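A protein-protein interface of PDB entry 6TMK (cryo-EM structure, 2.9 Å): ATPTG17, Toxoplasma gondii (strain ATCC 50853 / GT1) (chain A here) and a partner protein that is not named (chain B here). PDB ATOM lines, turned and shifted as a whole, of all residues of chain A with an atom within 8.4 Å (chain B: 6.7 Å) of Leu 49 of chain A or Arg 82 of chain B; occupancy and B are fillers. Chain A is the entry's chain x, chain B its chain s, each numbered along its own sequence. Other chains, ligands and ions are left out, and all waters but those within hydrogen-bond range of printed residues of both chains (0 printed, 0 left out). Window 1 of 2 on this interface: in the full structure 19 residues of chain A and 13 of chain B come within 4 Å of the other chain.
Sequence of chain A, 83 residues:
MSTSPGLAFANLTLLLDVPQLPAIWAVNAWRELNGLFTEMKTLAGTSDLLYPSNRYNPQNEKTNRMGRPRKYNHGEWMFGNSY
O of Thr 46 of chain A is in hydrogen-bond range of NH2 of Arg 82 of chain B, 3.1 Å away. The backbone carbonyl oxygen of Ser 47 of chain A sits at hydrogen-bond distance from the guanidinium group of Arg 82 of chain B. The side-chain hydroxyl of Tyr 51 of chain A sits at hydrogen-bond distance from the side-chain carboxylate of Glu 83 of chain B (3.2 Å). The guanidinium group (NH2) of Arg 65 of chain A sits at hydrogen-bond distance from the side-chain hydroxyl (OG) of Ser 86 of chain B, 3.2 Å away.
The backbone carbonyl oxygen of Asp 48 of chain A sits at hydrogen-bond distance from the side-chain hydroxyl of Thr 46 of chain A. ND2 of Asn 81 of chain A is in hydrogen-bond range of OG of Ser 47 of chain A, at 3.4 Å. OG of Ser 47 of chain A is in hydrogen-bond range of OH of Tyr 83 of chain A, 3.0 Å away. The side-chain carboxylate of Asp 48 of chain A is in salt-bridge range of the guanidinium group of Arg 70 of chain A (2.8 Å). The backbone carbonyl oxygen (O) of Leu 49 of chain A lies within hydrogen-bond range of the side-chain amide nitrogen (NE2) of Gln 59 of chain A (2.8 Å). The side-chain amide nitrogen (ND2) of Asn 57 of chain A is in hydrogen-bond range of the backbone carbonyl oxygen (O) of Tyr 51 of chain A (2.8 Å).
Among the printed residues, merely in contact across the chains: Tyr 83 of chain A with Ser 86 of chain B, Pro 52 of chain A with Leu 79 of chain B, Leu 50 of chain A with Leu 79 of chain B, Asp 48 of chain A with Arg 82 of chain B, Leu 49 of chain A with Glu 83 of chain B, Leu 49 of chain A with Arg 82 of chain B, Leu 49 of chain A with Leu 79 of chain B and Arg 65 of chain A with Glu 83 of chain B.
Leu 49 of chain A touches three residues of chain B. Arg 82 of chain B touches four residues of chain A. Of the printed residues of chain A, Glu 83 of chain B touches Leu 49, Tyr 51 and Arg 65. Printed residues of chain B within 4 Å of Leu 50 of chain A: Leu 79 (3.7 Å). Printed residues of chain B within 4 Å of Thr 46 of chain A: Arg 82 (3.1 Å). The nearest residue of chain B that does not touch Leu 49 of chain A is Ser 86 of chain B (4.9 Å). The nearest printed residue of chain A that does not touch Glu 83 of chain B is Tyr 83 of chain A (7.2 Å).
Of the 11 printed residues of chain B, 4 touch a printed residue of chain A. Of the 22 printed residues of chain A, 9 touch a printed residue of chain B. Among the printed residues, 12 pairs touch across the chains. Among the printed residues, no Asp or Glu carboxylate lies within 4 Å of a Lys or Arg side-chain nitrogen of the other chain.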
ATOM      1  N   THR A  38      10.209 -35.129   1.553  1.00  0.00           N
ATOM      2  CA  THR A  38       9.569 -34.389   0.474  1.00  0.00           C
ATOM      3  C   THR A  38      10.595 -33.893  -0.533  1.00  0.00           C
ATOM      4  O   THR A  38      10.381 -33.982  -1.748  1.00  0.00           O
ATOM      5  CB  THR A  38       8.780 -33.216   1.050  1.00  0.00           C
ATOM      6  OG1 THR A  38       7.866 -33.694   2.042  1.00  0.00           O
ATOM      7  CG2 THR A  38       8.016 -32.501  -0.042  1.00  0.00           C
ATOM      8  N   LYS A  41      11.908 -36.795  -2.619  1.00  0.00           N
ATOM      9  CA  LYS A  41      10.922 -37.140  -3.637  1.00  0.00           C
ATOM     10  C   LYS A  41      10.961 -36.149  -4.792  1.00  0.00           C
ATOM     11  O   LYS A  41      10.933 -36.537  -5.967  1.00  0.00           O
ATOM     12  CB  LYS A  41       9.533 -37.199  -3.011  1.00  0.00           C
ATOM     13  CG  LYS A  41       8.442 -37.624  -3.961  1.00  0.00           C
ATOM     14  CD  LYS A  41       7.366 -38.396  -3.232  1.00  0.00           C
ATOM     15  CE  LYS A  41       6.789 -37.593  -2.086  1.00  0.00           C
ATOM     16  NZ  LYS A  41       5.462 -38.115  -1.660  1.00  0.00           N
ATOM     17  N   THR A  42      11.021 -34.856  -4.473  1.00  0.00           N
ATOM     18  CA  THR A  42      11.081 -33.839  -5.517  1.00  0.00           C
ATOM     19  C   THR A  42      12.324 -34.002  -6.382  1.00  0.00           C
ATOM     20  O   THR A  42      12.255 -33.866  -7.609  1.00  0.00           O
ATOM     21  CB  THR A  42      11.055 -32.449  -4.888  1.00  0.00           C
ATOM     22  OG1 THR A  42       9.843 -32.278  -4.148  1.00  0.00           O
ATOM     23  CG2 THR A  42      11.157 -31.388  -5.947  1.00  0.00           C
ATOM     24  N   LEU A  43      13.468 -34.288  -5.765  1.00  0.00           N
ATOM     25  CA  LEU A  43      14.683 -34.512  -6.540  1.00  0.00           C
ATOM     26  C   LEU A  43      14.545 -35.738  -7.428  1.00  0.00           C
ATOM     27  O   LEU A  43      14.991 -35.734  -8.581  1.00  0.00           O
ATOM     28  CB  LEU A  43      15.880 -34.661  -5.611  1.00  0.00           C
ATOM     29  CG  LEU A  43      16.325 -33.383  -4.908  1.00  0.00           C
ATOM     30  CD1 LEU A  43      17.267 -33.717  -3.781  1.00  0.00           C
ATOM     31  CD2 LEU A  43      16.989 -32.449  -5.888  1.00  0.00           C
ATOM     32  N   GLY A  45      11.807 -36.909  -8.747  1.00  0.00           N
ATOM     33  CA  GLY A  45      10.976 -36.462  -9.850  1.00  0.00           C
ATOM     34  C   GLY A  45       9.509 -36.740  -9.609  1.00  0.00           C
ATOM     35  O   GLY A  45       9.133 -37.716  -8.957  1.00  0.00           O
ATOM     36  N   THR A  46       8.664 -35.866 -10.147  1.00  0.00           N
ATOM     37  CA  THR A  46       7.223 -35.966  -9.993  1.00  0.00           C
ATOM     38  C   THR A  46       6.551 -35.599 -11.305  1.00  0.00           C
ATOM     39  O   THR A  46       7.086 -34.821 -12.099  1.00  0.00           O
ATOM     40  CB  THR A  46       6.705 -35.047  -8.877  1.00  0.00           C
ATOM     41  OG1 THR A  46       6.990 -33.681  -9.206  1.00  0.00           O
ATOM     42  CG2 THR A  46       7.349 -35.387  -7.555  1.00  0.00           C
ATOM     43  N   SER A  47       5.372 -36.177 -11.528  1.00  0.00           N
ATOM     44  CA  SER A  47       4.571 -35.794 -12.682  1.00  0.00           C
ATOM     45  C   SER A  47       4.087 -34.358 -12.538  1.00  0.00           C
ATOM     46  O   SER A  47       4.396 -33.497 -13.368  1.00  0.00           O
ATOM     47  CB  SER A  47       3.394 -36.755 -12.844  1.00  0.00           C
ATOM     48  OG  SER A  47       2.730 -36.539 -14.075  1.00  0.00           O
ATOM     49  N   ASP A  48       3.328 -34.082 -11.484  1.00  0.00           N
ATOM     50  CA  ASP A  48       2.987 -32.723 -11.098  1.00  0.00           C
ATOM     51  C   ASP A  48       3.829 -32.293  -9.904  1.00  0.00           C
ATOM     52  O   ASP A  48       4.365 -33.114  -9.157  1.00  0.00           O
ATOM     53  CB  ASP A  48       1.501 -32.606 -10.759  1.00  0.00           C
ATOM     54  CG  ASP A  48       0.988 -31.183 -10.869  1.00  0.00           C
ATOM     55  OD1 ASP A  48       1.811 -30.263 -11.044  1.00  0.00           O
ATOM     56  OD2 ASP A  48      -0.240 -30.982 -10.779  1.00  0.00           O
ATOM     57  N   LEU A  49       3.943 -30.981  -9.739  1.00  0.00           N
ATOM     58  CA  LEU A  49       4.815 -30.420  -8.724  1.00  0.00           C
ATOM     59  C   LEU A  49       4.310 -30.756  -7.325  1.00  0.00           C
ATOM     60  O   LEU A  49       3.187 -31.226  -7.126  1.00  0.00           O
ATOM     61  CB  LEU A  49       4.932 -28.907  -8.893  1.00  0.00           C
ATOM     62  CG  LEU A  49       3.647 -28.087  -8.939  1.00  0.00           C
ATOM     63  CD1 LEU A  49       3.151 -27.726  -7.559  1.00  0.00           C
ATOM     64  CD2 LEU A  49       3.883 -26.836  -9.744  1.00  0.00           C
ATOM     65  N   LEU A  50       5.171 -30.505  -6.343  1.00  0.00           N
ATOM     66  CA  LEU A  50       4.825 -30.587  -4.934  1.00  0.00           C
ATOM     67  C   LEU A  50       5.071 -29.239  -4.277  1.00  0.00           C
ATOM     68  O   LEU A  50       6.139 -28.645  -4.450  1.00  0.00           O
ATOM     69  CB  LEU A  50       5.636 -31.664  -4.217  1.00  0.00           C
ATOM     70  CG  LEU A  50       5.478 -33.102  -4.699  1.00  0.00           C
ATOM     71  CD1 LEU A  50       6.401 -33.991  -3.909  1.00  0.00           C
ATOM     72  CD2 LEU A  50       4.046 -33.575  -4.574  1.00  0.00           C
ATOM     73  N   TYR A  51       4.085 -28.764  -3.533  1.00  0.00           N
ATOM     74  CA  TYR A  51       4.268 -27.580  -2.711  1.00  0.00           C
ATOM     75  C   TYR A  51       4.963 -27.981  -1.415  1.00  0.00           C
ATOM     76  O   TYR A  51       4.404 -28.773  -0.650  1.00  0.00           O
ATOM     77  CB  TYR A  51       2.933 -26.930  -2.399  1.00  0.00           C
ATOM     78  CG  TYR A  51       2.173 -26.408  -3.590  1.00  0.00           C
ATOM     79  CD1 TYR A  51       2.681 -25.390  -4.369  1.00  0.00           C
ATOM     80  CD2 TYR A  51       0.934 -26.924  -3.922  1.00  0.00           C
ATOM     81  CE1 TYR A  51       1.985 -24.908  -5.450  1.00  0.00           C
ATOM     82  CE2 TYR A  51       0.234 -26.449  -4.999  1.00  0.00           C
ATOM     83  CZ  TYR A  51       0.763 -25.439  -5.760  1.00  0.00           C
ATOM     84  OH  TYR A  51       0.069 -24.958  -6.842  1.00  0.00           O
ATOM     85  N   PRO A  52       6.162 -27.469  -1.125  1.00  0.00           N
ATOM     86  CA  PRO A  52       6.918 -27.992   0.019  1.00  0.00           C
ATOM     87  C   PRO A  52       6.291 -27.665   1.363  1.00  0.00           C
ATOM     88  O   PRO A  52       6.112 -28.553   2.202  1.00  0.00           O
ATOM     89  CB  PRO A  52       8.289 -27.317  -0.125  1.00  0.00           C
ATOM     90  CG  PRO A  52       8.269 -26.592  -1.405  1.00  0.00           C
ATOM     91  CD  PRO A  52       6.859 -26.341  -1.756  1.00  0.00           C
ATOM     92  N   ASN A  54       3.353 -26.923   2.230  1.00  0.00           N
ATOM     93  CA  ASN A  54       1.926 -27.166   2.316  1.00  0.00           C
ATOM     94  C   ASN A  54       1.646 -28.457   3.072  1.00  0.00           C
ATOM     95  O   ASN A  54       2.470 -29.374   3.108  1.00  0.00           O
ATOM     96  CB  ASN A  54       1.320 -27.239   0.918  1.00  0.00           C
ATOM     97  CG  ASN A  54       1.300 -25.898   0.220  1.00  0.00           C
ATOM     98  OD1 ASN A  54       2.259 -25.133   0.289  1.00  0.00           O
ATOM     99  ND2 ASN A  54       0.209 -25.610  -0.469  1.00  0.00           N
ATOM    100  N   ASN A  57      -0.369 -32.858  -0.305  1.00  0.00           N
ATOM    101  CA  ASN A  57      -0.182 -32.744  -1.749  1.00  0.00           C
ATOM    102  C   ASN A  57      -0.780 -33.975  -2.413  1.00  0.00           C
ATOM    103  O   ASN A  57      -0.080 -34.970  -2.639  1.00  0.00           O
ATOM    104  CB  ASN A  57       1.293 -32.601  -2.106  1.00  0.00           C
ATOM    105  CG  ASN A  57       1.771 -31.173  -2.053  1.00  0.00           C
ATOM    106  OD1 ASN A  57       1.437 -30.359  -2.910  1.00  0.00           O
ATOM    107  ND2 ASN A  57       2.561 -30.860  -1.045  1.00  0.00           N
ATOM    108  N   PRO A  58      -2.070 -33.949  -2.746  1.00  0.00           N
ATOM    109  CA  PRO A  58      -2.701 -35.120  -3.362  1.00  0.00           C
ATOM    110  C   PRO A  58      -2.583 -35.214  -4.875  1.00  0.00           C
ATOM    111  O   PRO A  58      -3.076 -36.192  -5.448  1.00  0.00           O
ATOM    112  CB  PRO A  58      -4.166 -34.937  -2.960  1.00  0.00           C
ATOM    113  CG  PRO A  58      -4.348 -33.474  -2.908  1.00  0.00           C
ATOM    114  CD  PRO A  58      -3.045 -32.876  -2.489  1.00  0.00           C
ATOM    115  N   GLN A  59      -1.946 -34.253  -5.530  1.00  0.00           N
ATOM    116  CA  GLN A  59      -1.975 -34.195  -6.983  1.00  0.00           C
ATOM    117  C   GLN A  59      -1.202 -35.348  -7.607  1.00  0.00           C
ATOM    118  O   GLN A  59      -0.099 -35.691  -7.174  1.00  0.00           O
ATOM    119  CB  GLN A  59      -1.416 -32.864  -7.474  1.00  0.00           C
ATOM    120  CG  GLN A  59      -0.062 -32.524  -6.938  1.00  0.00           C
ATOM    121  CD  GLN A  59      -0.125 -31.616  -5.743  1.00  0.00           C
ATOM    122  OE1 GLN A  59      -1.148 -31.519  -5.072  1.00  0.00           O
ATOM    123  NE2 GLN A  59       0.974 -30.949  -5.463  1.00  0.00           N
ATOM    124  N   ASN A  60      -1.796 -35.947  -8.631  1.00  0.00           N
ATOM    125  CA  ASN A  60      -1.151 -36.990  -9.414  1.00  0.00           C
ATOM    126  C   ASN A  60      -1.714 -36.904 -10.828  1.00  0.00           C
ATOM    127  O   ASN A  60      -2.285 -35.882 -11.219  1.00  0.00           O
ATOM    128  CB  ASN A  60      -1.355 -38.370  -8.769  1.00  0.00           C
ATOM    129  CG  ASN A  60      -2.785 -38.839  -8.827  1.00  0.00           C
ATOM    130  OD1 ASN A  60      -3.314 -39.125  -9.900  1.00  0.00           O
ATOM    131  ND2 ASN A  60      -3.414 -38.950  -7.672  1.00  0.00           N
ATOM    132  N   ASN A  64      -6.483 -33.639  -8.990  1.00  0.00           N
ATOM    133  CA  ASN A  64      -6.143 -32.229  -8.930  1.00  0.00           C
ATOM    134  C   ASN A  64      -5.286 -31.926  -7.705  1.00  0.00           C
ATOM    135  O   ASN A  64      -5.044 -32.775  -6.846  1.00  0.00           O
ATOM    136  CB  ASN A  64      -7.412 -31.375  -8.902  1.00  0.00           C
ATOM    137  CG  ASN A  64      -7.831 -30.913 -10.267  1.00  0.00           C
ATOM    138  OD1 ASN A  64      -7.079 -31.012 -11.234  1.00  0.00           O
ATOM    139  ND2 ASN A  64      -9.038 -30.393 -10.354  1.00  0.00           N
ATOM    140  N   ARG A  65      -4.839 -30.679  -7.630  1.00  0.00           N
ATOM    141  CA  ARG A  65      -4.150 -30.163  -6.459  1.00  0.00           C
ATOM    142  C   ARG A  65      -5.090 -29.827  -5.314  1.00  0.00           C
ATOM    143  O   ARG A  65      -4.650 -29.230  -4.330  1.00  0.00           O
ATOM    144  CB  ARG A  65      -3.340 -28.929  -6.841  1.00  0.00           C
ATOM    145  CG  ARG A  65      -2.253 -29.225  -7.824  1.00  0.00           C
ATOM    146  CD  ARG A  65      -1.503 -27.997  -8.245  1.00  0.00           C
ATOM    147  NE  ARG A  65      -0.640 -28.270  -9.386  1.00  0.00           N
ATOM    148  CZ  ARG A  65       0.062 -27.349 -10.030  1.00  0.00           C
ATOM    149  NH1 ARG A  65       0.011 -26.088  -9.646  1.00  0.00           N
ATOM    150  NH2 ARG A  65       0.816 -27.690 -11.060  1.00  0.00           N
ATOM    151  N   ARG A  70      -9.097 -34.783 -12.214  1.00  0.00           N
ATOM    152  CA  ARG A  70      -8.707 -33.806 -13.217  1.00  0.00           C
ATOM    153  C   ARG A  70      -9.728 -33.763 -14.343  1.00  0.00           C
ATOM    154  O   ARG A  70     -10.174 -34.802 -14.836  1.00  0.00           O
ATOM    155  CB  ARG A  70      -7.329 -34.141 -13.770  1.00  0.00           C
ATOM    156  CG  ARG A  70      -6.194 -33.670 -12.912  1.00  0.00           C
ATOM    157  CD  ARG A  70      -4.865 -33.980 -13.544  1.00  0.00           C
ATOM    158  NE  ARG A  70      -3.769 -33.934 -12.586  1.00  0.00           N
ATOM    159  CZ  ARG A  70      -3.217 -32.817 -12.135  1.00  0.00           C
ATOM    160  NH1 ARG A  70      -3.648 -31.641 -12.544  1.00  0.00           N
ATOM    161  NH2 ARG A  70      -2.227 -32.878 -11.268  1.00  0.00           N
ATOM    162  N   ASN A  81       1.753 -33.767 -20.634  1.00  0.00           N
ATOM    163  CA  ASN A  81       0.872 -33.546 -19.499  1.00  0.00           C
ATOM    164  C   ASN A  81       0.124 -32.231 -19.655  1.00  0.00           C
ATOM    165  O   ASN A  81       0.622 -31.270 -20.245  1.00  0.00           O
ATOM    166  CB  ASN A  81       1.667 -33.544 -18.200  1.00  0.00           C
ATOM    167  CG  ASN A  81       2.088 -34.928 -17.776  1.00  0.00           C
ATOM    168  OD1 ASN A  81       1.386 -35.907 -18.030  1.00  0.00           O
ATOM    169  ND2 ASN A  81       3.237 -35.021 -17.119  1.00  0.00           N
ATOM    170  N   TYR A  83      -0.410 -30.078 -17.511  1.00  0.00           N
ATOM    171  CA  TYR A  83      -0.061 -29.285 -16.346  1.00  0.00           C
ATOM    172  C   TYR A  83       1.448 -29.126 -16.222  1.00  0.00           C
ATOM    173  O   TYR A  83       2.198 -29.546 -17.099  1.00  0.00           O
ATOM    174  CB  TYR A  83      -0.645 -29.913 -15.079  1.00  0.00           C
ATOM    175  CG  TYR A  83      -0.485 -31.408 -14.977  1.00  0.00           C
ATOM    176  CD1 TYR A  83      -1.541 -32.252 -15.261  1.00  0.00           C
ATOM    177  CD2 TYR A  83       0.711 -31.973 -14.584  1.00  0.00           C
ATOM    178  CE1 TYR A  83      -1.407 -33.613 -15.168  1.00  0.00           C
ATOM    179  CE2 TYR A  83       0.851 -33.335 -14.488  1.00  0.00           C
ATOM    180  CZ  TYR A  83      -0.210 -34.151 -14.780  1.00  0.00           C
ATOM    181  OH  TYR A  83      -0.073 -35.514 -14.684  1.00  0.00           O
ATOM    182  N   ARG B  77      12.349 -20.737  -6.018  1.00  0.00           N
ATOM    183  CA  ARG B  77      12.520 -20.139  -7.336  1.00  0.00           C
ATOM    184  C   ARG B  77      12.161 -21.134  -8.437  1.00  0.00           C
ATOM    185  O   ARG B  77      11.348 -20.840  -9.334  1.00  0.00           O
ATOM    186  CB  ARG B  77      13.956 -19.651  -7.482  1.00  0.00           C
ATOM    187  CG  ARG B  77      14.118 -18.435  -8.342  1.00  0.00           C
ATOM    188  CD  ARG B  77      15.531 -17.917  -8.288  1.00  0.00           C
ATOM    189  NE  ARG B  77      15.751 -17.116  -7.085  1.00  0.00           N
ATOM    190  CZ  ARG B  77      16.670 -17.363  -6.155  1.00  0.00           C
ATOM    191  NH1 ARG B  77      17.489 -18.400  -6.250  1.00  0.00           N
ATOM    192  NH2 ARG B  77      16.764 -16.564  -5.107  1.00  0.00           N
ATOM    193  N   LYS B  78      12.763 -22.325  -8.383  1.00  0.00           N
ATOM    194  CA  LYS B  78      12.448 -23.344  -9.380  1.00  0.00           C
ATOM    195  C   LYS B  78      10.962 -23.673  -9.388  1.00  0.00           C
ATOM    196  O   LYS B  78      10.354 -23.851 -10.454  1.00  0.00           O
ATOM    197  CB  LYS B  78      13.264 -24.606  -9.123  1.00  0.00           C
ATOM    198  CG  LYS B  78      14.751 -24.435  -9.292  1.00  0.00           C
ATOM    199  CD  LYS B  78      15.473 -25.728  -8.972  1.00  0.00           C
ATOM    200  CE  LYS B  78      16.917 -25.499  -8.578  1.00  0.00           C
ATOM    201  NZ  LYS B  78      17.453 -26.653  -7.798  1.00  0.00           N
ATOM    202  N   LEU B  79      10.361 -23.760  -8.204  1.00  0.00           N
ATOM    203  CA  LEU B  79       8.958 -24.128  -8.100  1.00  0.00           C
ATOM    204  C   LEU B  79       8.060 -23.055  -8.690  1.00  0.00           C
ATOM    205  O   LEU B  79       7.041 -23.368  -9.310  1.00  0.00           O
ATOM    206  CB  LEU B  79       8.613 -24.389  -6.640  1.00  0.00           C
ATOM    207  CG  LEU B  79       7.157 -24.657  -6.312  1.00  0.00           C
ATOM    208  CD1 LEU B  79       6.693 -25.945  -6.933  1.00  0.00           C
ATOM    209  CD2 LEU B  79       7.030 -24.712  -4.826  1.00  0.00           C
ATOM    210  N   ASN B  80       8.402 -21.786  -8.482  1.00  0.00           N
ATOM    211  CA  ASN B  80       7.628 -20.701  -9.067  1.00  0.00           C
ATOM    212  C   ASN B  80       7.657 -20.783 -10.586  1.00  0.00           C
ATOM    213  O   ASN B  80       6.620 -20.652 -11.255  1.00  0.00           O
ATOM    214  CB  ASN B  80       8.194 -19.371  -8.579  1.00  0.00           C
ATOM    215  CG  ASN B  80       7.302 -18.204  -8.891  1.00  0.00           C
ATOM    216  OD1 ASN B  80       6.100 -18.235  -8.641  1.00  0.00           O
ATOM    217  ND2 ASN B  80       7.892 -17.156  -9.435  1.00  0.00           N
ATOM    218  N   GLU B  81       8.847 -21.007 -11.146  1.00  0.00           N
ATOM    219  CA  GLU B  81       8.960 -21.192 -12.592  1.00  0.00           C
ATOM    220  C   GLU B  81       8.056 -22.321 -13.076  1.00  0.00           C
ATOM    221  O   GLU B  81       7.260 -22.152 -14.018  1.00  0.00           O
ATOM    222  CB  GLU B  81      10.414 -21.468 -12.959  1.00  0.00           C
ATOM    223  CG  GLU B  81      10.695 -21.467 -14.436  1.00  0.00           C
ATOM    224  CD  GLU B  81      12.176 -21.386 -14.742  1.00  0.00           C
ATOM    225  OE1 GLU B  81      12.777 -20.320 -14.497  1.00  0.00           O
ATOM    226  OE2 GLU B  81      12.741 -22.391 -15.221  1.00  0.00           O
ATOM    227  N   ARG B  82       8.165 -23.485 -12.434  1.00  0.00           N
ATOM    228  CA  ARG B  82       7.381 -24.640 -12.849  1.00  0.00           C
ATOM    229  C   ARG B  82       5.889 -24.369 -12.734  1.00  0.00           C
ATOM    230  O   ARG B  82       5.112 -24.769 -13.605  1.00  0.00           O
ATOM    231  CB  ARG B  82       7.766 -25.861 -12.019  1.00  0.00           C
ATOM    232  CG  ARG B  82       6.967 -27.096 -12.356  1.00  0.00           C
ATOM    233  CD  ARG B  82       7.683 -28.363 -11.975  1.00  0.00           C
ATOM    234  NE  ARG B  82       6.970 -29.542 -12.449  1.00  0.00           N
ATOM    235  CZ  ARG B  82       7.192 -30.774 -12.011  1.00  0.00           C
ATOM    236  NH1 ARG B  82       8.108 -30.995 -11.085  1.00  0.00           N
ATOM    237  NH2 ARG B  82       6.493 -31.785 -12.498  1.00  0.00           N
ATOM    238  N   GLU B  83       5.468 -23.701 -11.664  1.00  0.00           N
ATOM    239  CA  GLU B  83       4.051 -23.442 -11.456  1.00  0.00           C
ATOM    240  C   GLU B  83       3.498 -22.526 -12.536  1.00  0.00           C
ATOM    241  O   GLU B  83       2.405 -22.769 -13.067  1.00  0.00           O
ATOM    242  CB  GLU B  83       3.839 -22.827 -10.077  1.00  0.00           C
ATOM    243  CG  GLU B  83       2.415 -22.902  -9.582  1.00  0.00           C
ATOM    244  CD  GLU B  83       2.086 -21.849  -8.538  1.00  0.00           C
ATOM    245  OE1 GLU B  83       2.803 -20.829  -8.464  1.00  0.00           O
ATOM    246  OE2 GLU B  83       1.102 -22.039  -7.794  1.00  0.00           O
ATOM    247  N   ILE B  84       4.235 -21.470 -12.874  1.00  0.00           N
ATOM    248  CA  ILE B  84       3.784 -20.576 -13.936  1.00  0.00           C
ATOM    249  C   ILE B  84       3.624 -21.342 -15.242  1.00  0.00           C
ATOM    250  O   ILE B  84       2.588 -21.250 -15.920  1.00  0.00           O
ATOM    251  CB  ILE B  84       4.756 -19.394 -14.090  1.00  0.00           C
ATOM    252  CG1 ILE B  84       4.698 -18.513 -12.853  1.00  0.00           C
ATOM    253  CG2 ILE B  84       4.415 -18.590 -15.303  1.00  0.00           C
ATOM    254  CD1 ILE B  84       5.855 -17.618 -12.692  1.00  0.00           C
ATOM    255  N   ILE B  85       4.648 -22.111 -15.618  1.00  0.00           N
ATOM    256  CA  ILE B  85       4.581 -22.797 -16.904  1.00  0.00           C
ATOM    257  C   ILE B  85       3.483 -23.851 -16.909  1.00  0.00           C
ATOM    258  O   ILE B  85       2.821 -24.064 -17.933  1.00  0.00           O
ATOM    259  CB  ILE B  85       5.953 -23.390 -17.255  1.00  0.00           C
ATOM    260  CG1 ILE B  85       6.944 -22.256 -17.481  1.00  0.00           C
ATOM    261  CG2 ILE B  85       5.855 -24.278 -18.468  1.00  0.00           C
ATOM    262  CD1 ILE B  85       8.355 -22.685 -17.532  1.00  0.00           C
ATOM    263  N   SER B  86       3.239 -24.496 -15.772  1.00  0.00           N
ATOM    264  CA  SER B  86       2.183 -25.494 -15.682  1.00  0.00           C
ATOM    265  C   SER B  86       0.814 -24.856 -15.870  1.00  0.00           C
ATOM    266  O   SER B  86      -0.037 -25.381 -16.602  1.00  0.00           O
ATOM    267  CB  SER B  86       2.278 -26.207 -14.339  1.00  0.00           C
ATOM    268  OG  SER B  86       1.202 -27.101 -14.141  1.00  0.00           O
ATOM    269  N   ASP B  87       0.580 -23.728 -15.206  1.00  0.00           N
ATOM    270  CA  ASP B  87      -0.702 -23.055 -15.349  1.00  0.00           C
ATOM    271  C   ASP B  87      -0.921 -22.606 -16.785  1.00  0.00           C
ATOM    272  O   ASP B  87      -2.034 -22.715 -17.320  1.00  0.00           O
ATOM    273  CB  ASP B  87      -0.772 -21.871 -14.393  1.00  0.00           C
ATOM    274  CG  ASP B  87      -0.841 -22.298 -12.943  1.00  0.00           C
ATOM    275  OD1 ASP B  87      -0.285 -21.579 -12.086  1.00  0.00           O
ATOM    276  OD2 ASP B  87      -1.441 -23.356 -12.657  1.00  0.00           O
